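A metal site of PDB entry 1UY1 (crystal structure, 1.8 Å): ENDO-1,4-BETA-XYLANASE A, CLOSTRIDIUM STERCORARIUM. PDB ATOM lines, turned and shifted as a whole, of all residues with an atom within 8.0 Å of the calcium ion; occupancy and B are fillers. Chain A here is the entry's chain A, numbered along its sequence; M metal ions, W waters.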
ATOM      1  N   ILE A  23     -17.253  22.169  19.395  1.00  0.00           N
ATOM      2  CA  ILE A  23     -17.871  22.991  18.358  1.00  0.00           C
ATOM      3  C   ILE A  23     -16.767  23.751  17.626  1.00  0.00           C
ATOM      4  O   ILE A  23     -15.860  24.345  18.256  1.00  0.00           O
ATOM      5  CB  ILE A  23     -18.863  24.004  18.988  1.00  0.00           C
ATOM      6  CG1 ILE A  23     -20.123  23.301  19.502  1.00  0.00           C
ATOM      7  CG2 ILE A  23     -19.210  25.148  17.971  1.00  0.00           C
ATOM      8  CD1 ILE A  23     -21.022  22.700  18.434  1.00  0.00           C
ATOM      9  N   ILE A  24     -16.837  23.710  16.297  1.00  0.00           N
ATOM     10  CA  ILE A  24     -15.941  24.466  15.442  1.00  0.00           C
ATOM     11  C   ILE A  24     -16.793  25.516  14.817  1.00  0.00           C
ATOM     12  O   ILE A  24     -17.859  25.223  14.314  1.00  0.00           O
ATOM     13  CB  ILE A  24     -15.310  23.539  14.362  1.00  0.00           C
ATOM     14  CG1 ILE A  24     -14.406  22.494  15.040  1.00  0.00           C
ATOM     15  CG2 ILE A  24     -14.481  24.370  13.366  1.00  0.00           C
ATOM     16  CD1 ILE A  24     -14.110  21.276  14.145  1.00  0.00           C
ATOM     17  N   GLU A  25     -16.376  26.780  14.948  1.00  0.00           N
ATOM     18  CA  GLU A  25     -17.099  27.911  14.342  1.00  0.00           C
ATOM     19  C   GLU A  25     -16.774  28.058  12.866  1.00  0.00           C
ATOM     20  O   GLU A  25     -15.629  28.187  12.479  1.00  0.00           O
ATOM     21  CB  GLU A  25     -16.801  29.202  15.099  1.00  0.00           C
ATOM     22  CG  GLU A  25     -17.209  29.106  16.589  1.00  0.00           C
ATOM     23  CD  GLU A  25     -18.708  29.085  16.787  1.00  0.00           C
ATOM     24  OE1 GLU A  25     -19.528  29.242  15.788  1.00  0.00           O
ATOM     25  OE2 GLU A  25     -19.085  28.882  17.922  1.00  0.00           O
ATOM     26  N   ALA A  26     -17.815  28.044  12.026  1.00  0.00           N
ATOM     27  CA  ALA A  26     -17.624  28.117  10.597  1.00  0.00           C
ATOM     28  C   ALA A  26     -16.918  29.417  10.136  1.00  0.00           C
ATOM     29  O   ALA A  26     -16.126  29.409   9.168  1.00  0.00           O
ATOM     30  CB  ALA A  26     -18.953  27.942   9.872  1.00  0.00           C
ATOM     31  N   GLU A  27     -17.214  30.513  10.835  1.00  0.00           N
ATOM     32  CA  GLU A  27     -16.617  31.811  10.574  1.00  0.00           C
ATOM     33  C   GLU A  27     -15.139  31.912  10.924  1.00  0.00           C
ATOM     34  O   GLU A  27     -14.478  32.880  10.556  1.00  0.00           O
ATOM     35  CB  GLU A  27     -17.397  32.927  11.324  1.00  0.00           C
ATOM     36  CG  GLU A  27     -17.338  32.833  12.853  1.00  0.00           C
ATOM     37  CD  GLU A  27     -18.487  32.039  13.433  1.00  0.00           C
ATOM     38  OE1 GLU A  27     -19.052  31.150  12.728  1.00  0.00           O
ATOM     39  OE2 GLU A  27     -18.840  32.295  14.617  1.00  0.00           O
ATOM     40  N   GLU A  28     -14.619  30.953  11.667  1.00  0.00           N
ATOM     41  CA  GLU A  28     -13.203  30.841  11.977  1.00  0.00           C
ATOM     42  C   GLU A  28     -12.483  29.876  11.021  1.00  0.00           C
ATOM     43  O   GLU A  28     -11.776  28.953  11.399  1.00  0.00           O
ATOM     44  CB  GLU A  28     -13.064  30.443  13.452  1.00  0.00           C
ATOM     45  CG  GLU A  28     -13.652  31.514  14.372  1.00  0.00           C
ATOM     46  CD  GLU A  28     -13.523  31.191  15.837  1.00  0.00           C
ATOM     47  OE1 GLU A  28     -14.040  31.986  16.656  1.00  0.00           O
ATOM     48  OE2 GLU A  28     -12.930  30.156  16.188  1.00  0.00           O
ATOM     49  N   VAL A  39     -18.580  36.891   6.594  1.00  0.00           N
ATOM     50  CA  VAL A  39     -18.991  36.598   7.967  1.00  0.00           C
ATOM     51  C   VAL A  39     -20.298  37.374   8.206  1.00  0.00           C
ATOM     52  O   VAL A  39     -20.396  38.591   7.917  1.00  0.00           O
ATOM     53  CB  VAL A  39     -17.908  36.945   8.981  1.00  0.00           C
ATOM     54  CG1 VAL A  39     -18.417  36.767  10.429  1.00  0.00           C
ATOM     55  CG2 VAL A  39     -16.689  36.094   8.711  1.00  0.00           C
ATOM     56  N   ILE A  40     -21.312  36.639   8.652  1.00  0.00           N
ATOM     57  CA  ILE A  40     -22.646  37.149   8.872  1.00  0.00           C
ATOM     58  C   ILE A  40     -23.026  36.979  10.359  1.00  0.00           C
ATOM     59  O   ILE A  40     -22.447  36.174  11.070  1.00  0.00           O
ATOM     60  CB  ILE A  40     -23.652  36.449   7.959  1.00  0.00           C
ATOM     61  CG1 ILE A  40     -23.663  34.928   8.204  1.00  0.00           C
ATOM     62  CG2 ILE A  40     -23.385  36.799   6.504  1.00  0.00           C
ATOM     63  CD1 ILE A  40     -24.837  34.258   7.678  1.00  0.00           C
ATOM     64  N   THR A  42     -26.058  35.988  13.224  1.00  0.00           N
ATOM     65  CA  THR A  42     -27.205  35.062  13.395  1.00  0.00           C
ATOM     66  C   THR A  42     -28.209  35.657  14.351  1.00  0.00           C
ATOM     67  O   THR A  42     -27.879  36.634  15.008  1.00  0.00           O
ATOM     68  CB  THR A  42     -26.741  33.681  13.923  1.00  0.00           C
ATOM     69  OG1 THR A  42     -26.167  33.834  15.227  1.00  0.00           O
ATOM     70  CG2 THR A  42     -25.673  33.081  13.003  1.00  0.00           C
ATOM     71  N   GLY A  46     -24.825  35.419  17.283  1.00  0.00           N
ATOM     72  CA  GLY A  46     -23.640  34.638  16.959  1.00  0.00           C
ATOM     73  C   GLY A  46     -23.179  35.049  15.577  1.00  0.00           C
ATOM     74  O   GLY A  46     -23.616  36.073  15.038  1.00  0.00           O
ATOM     75  N   ARG A  47     -22.289  34.272  14.997  1.00  0.00           N
ATOM     76  CA  ARG A  47     -21.812  34.521  13.643  1.00  0.00           C
ATOM     77  C   ARG A  47     -21.803  33.232  12.842  1.00  0.00           C
ATOM     78  O   ARG A  47     -21.875  32.108  13.374  1.00  0.00           O
ATOM     79  CB  ARG A  47     -20.425  35.170  13.680  1.00  0.00           C
ATOM     80  CG  ARG A  47     -20.363  36.459  14.544  1.00  0.00           C
ATOM     81  CD  ARG A  47     -19.134  37.334  14.389  1.00  0.00           C
ATOM     82  NE  ARG A  47     -19.549  38.531  13.640  1.00  0.00           N
ATOM     83  CZ  ARG A  47     -18.754  39.279  12.828  1.00  0.00           C
ATOM     84  NH1 ARG A  47     -17.446  39.030  12.678  1.00  0.00           N
ATOM     85  NH2 ARG A  47     -19.301  40.313  12.161  1.00  0.00           N
ATOM     86  N   GLY A  48     -21.691  33.399  11.544  1.00  0.00           N
ATOM     87  CA  GLY A  48     -21.596  32.318  10.600  1.00  0.00           C
ATOM     88  C   GLY A  48     -20.968  32.807   9.309  1.00  0.00           C
ATOM     89  O   GLY A  48     -20.438  33.915   9.235  1.00  0.00           O
ATOM     90  N   ILE A  49     -20.965  31.927   8.321  1.00  0.00           N
ATOM     91  CA  ILE A  49     -20.563  32.304   6.989  1.00  0.00           C
ATOM     92  C   ILE A  49     -21.747  32.194   6.097  1.00  0.00           C
ATOM     93  O   ILE A  49     -22.579  31.315   6.252  1.00  0.00           O
ATOM     94  CB  ILE A  49     -19.363  31.441   6.474  1.00  0.00           C
ATOM     95  CG1 ILE A  49     -19.719  29.953   6.539  1.00  0.00           C
ATOM     96  CG2 ILE A  49     -18.151  31.697   7.336  1.00  0.00           C
ATOM     97  CD1 ILE A  49     -18.702  28.995   5.932  1.00  0.00           C
ATOM     98  N   THR A  75     -24.781  23.212  11.884  1.00  0.00           N
ATOM     99  CA  THR A  75     -25.926  24.047  12.100  1.00  0.00           C
ATOM    100  C   THR A  75     -26.006  25.057  10.982  1.00  0.00           C
ATOM    101  O   THR A  75     -25.123  25.948  10.856  1.00  0.00           O
ATOM    102  CB  THR A  75     -25.817  24.702  13.493  1.00  0.00           C
ATOM    103  OG1 THR A  75     -25.854  23.643  14.472  1.00  0.00           O
ATOM    104  CG2 THR A  75     -26.997  25.575  13.809  1.00  0.00           C
ATOM    105  N   TYR A 110     -32.011  28.406  11.555  1.00  0.00           N
ATOM    106  CA  TYR A 110     -30.949  27.389  11.633  1.00  0.00           C
ATOM    107  C   TYR A 110     -31.491  26.026  12.082  1.00  0.00           C
ATOM    108  O   TYR A 110     -32.456  25.936  12.845  1.00  0.00           O
ATOM    109  CB  TYR A 110     -29.792  27.890  12.486  1.00  0.00           C
ATOM    110  CG  TYR A 110     -29.037  28.972  11.750  1.00  0.00           C
ATOM    111  CD1 TYR A 110     -29.469  30.287  11.794  1.00  0.00           C
ATOM    112  CD2 TYR A 110     -27.909  28.659  10.984  1.00  0.00           C
ATOM    113  CE1 TYR A 110     -28.783  31.324  11.061  1.00  0.00           C
ATOM    114  CE2 TYR A 110     -27.205  29.665  10.289  1.00  0.00           C
ATOM    115  CZ  TYR A 110     -27.640  31.002  10.322  1.00  0.00           C
ATOM    116  OH  TYR A 110     -26.969  31.990   9.639  1.00  0.00           O
ATOM    117  N   VAL A 136     -23.837  28.874   7.352  1.00  0.00           N
ATOM    118  CA  VAL A 136     -23.296  27.895   8.330  1.00  0.00           C
ATOM    119  C   VAL A 136     -22.827  28.613   9.552  1.00  0.00           C
ATOM    120  O   VAL A 136     -21.967  29.492   9.478  1.00  0.00           O
ATOM    121  CB  VAL A 136     -22.124  27.097   7.738  1.00  0.00           C
ATOM    122  CG1 VAL A 136     -21.790  25.888   8.614  1.00  0.00           C
ATOM    123  CG2 VAL A 136     -22.442  26.641   6.303  1.00  0.00           C
ATOM    124  N   ASP A 137     -23.354  28.188  10.725  1.00  0.00           N
ATOM    125  CA  ASP A 137     -23.000  28.785  11.973  1.00  0.00           C
ATOM    126  C   ASP A 137     -21.766  28.013  12.559  1.00  0.00           C
ATOM    127  O   ASP A 137     -20.715  28.596  12.866  1.00  0.00           O
ATOM    128  CB  ASP A 137     -24.249  28.764  12.889  1.00  0.00           C
ATOM    129  CG  ASP A 137     -24.013  29.391  14.224  1.00  0.00           C
ATOM    130  OD1 ASP A 137     -22.844  29.515  14.651  1.00  0.00           O
ATOM    131  OD2 ASP A 137     -24.959  29.766  14.924  1.00  0.00           O
ATOM    132  N   ASN A 138     -21.904  26.712  12.656  1.00  0.00           N
ATOM    133  CA  ASN A 138     -20.899  25.854  13.338  1.00  0.00           C
ATOM    134  C   ASN A 138     -21.018  24.422  12.866  1.00  0.00           C
ATOM    135  O   ASN A 138     -21.949  24.097  12.118  1.00  0.00           O
ATOM    136  CB  ASN A 138     -20.968  26.004  14.856  1.00  0.00           C
ATOM    137  CG  ASN A 138     -22.253  25.434  15.474  1.00  0.00           C
ATOM    138  OD1 ASN A 138     -22.740  25.947  16.513  1.00  0.00           O
ATOM    139  ND2 ASN A 138     -22.755  24.346  14.939  1.00  0.00           N
ATOM    140  N   PHE A 139     -20.082  23.572  13.298  1.00  0.00           N
ATOM    141  CA  PHE A 139     -20.154  22.151  13.049  1.00  0.00           C
ATOM    142  C   PHE A 139     -19.307  21.401  14.036  1.00  0.00           C
ATOM    143  O   PHE A 139     -18.535  21.985  14.778  1.00  0.00           O
ATOM    144  CB  PHE A 139     -19.798  21.797  11.583  1.00  0.00           C
ATOM    145  CG  PHE A 139     -18.426  22.312  11.121  1.00  0.00           C
ATOM    146  CD1 PHE A 139     -18.308  23.524  10.415  1.00  0.00           C
ATOM    147  CD2 PHE A 139     -17.288  21.607  11.404  1.00  0.00           C
ATOM    148  CE1 PHE A 139     -17.065  23.991   9.956  1.00  0.00           C
ATOM    149  CE2 PHE A 139     -16.045  22.073  10.975  1.00  0.00           C
ATOM    150  CZ  PHE A 139     -15.949  23.265  10.241  1.00  0.00           C
HETATM  151 CA    CA M   1     -20.703  30.512  14.488  1.00  0.00          CA
HETATM  152  O   HOH W   1     -21.387  31.853  16.420  1.00  0.00           O
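The backbone carbonyl oxygen of Asp 137 sits close to the backbone NH of Ala 26, at 3.1 Å. The backbone NH (N) of Asp 137 lies within hydrogen-bond range of the backbone carbonyl oxygen (O) of Thr 75.
Of the 19 residues printed, 4 come within 4 Å of the calcium ion. Along chain A the residues within 4 Å of the calcium ion span positions 25 to 137.
The calcium ion is bound by OE1 of Glu 25 (2.2 Å). The backbone carbonyl oxygen (O) of Arg 47 binds the calcium ion. The calcium ion is bound by the side-chain carboxylate (OD1) of Asp 137 (2.4 Å). Water W1 binds the calcium ion. OE1 of Glu 27 is bound to the calcium ion (2.5 Å). The calcium ion is bound by O of Asp 137 (2.5 Å). OE2 of Glu 27 binds the calcium ion (2.6 Å). The calcium ion has seven donor atoms within binding distance.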
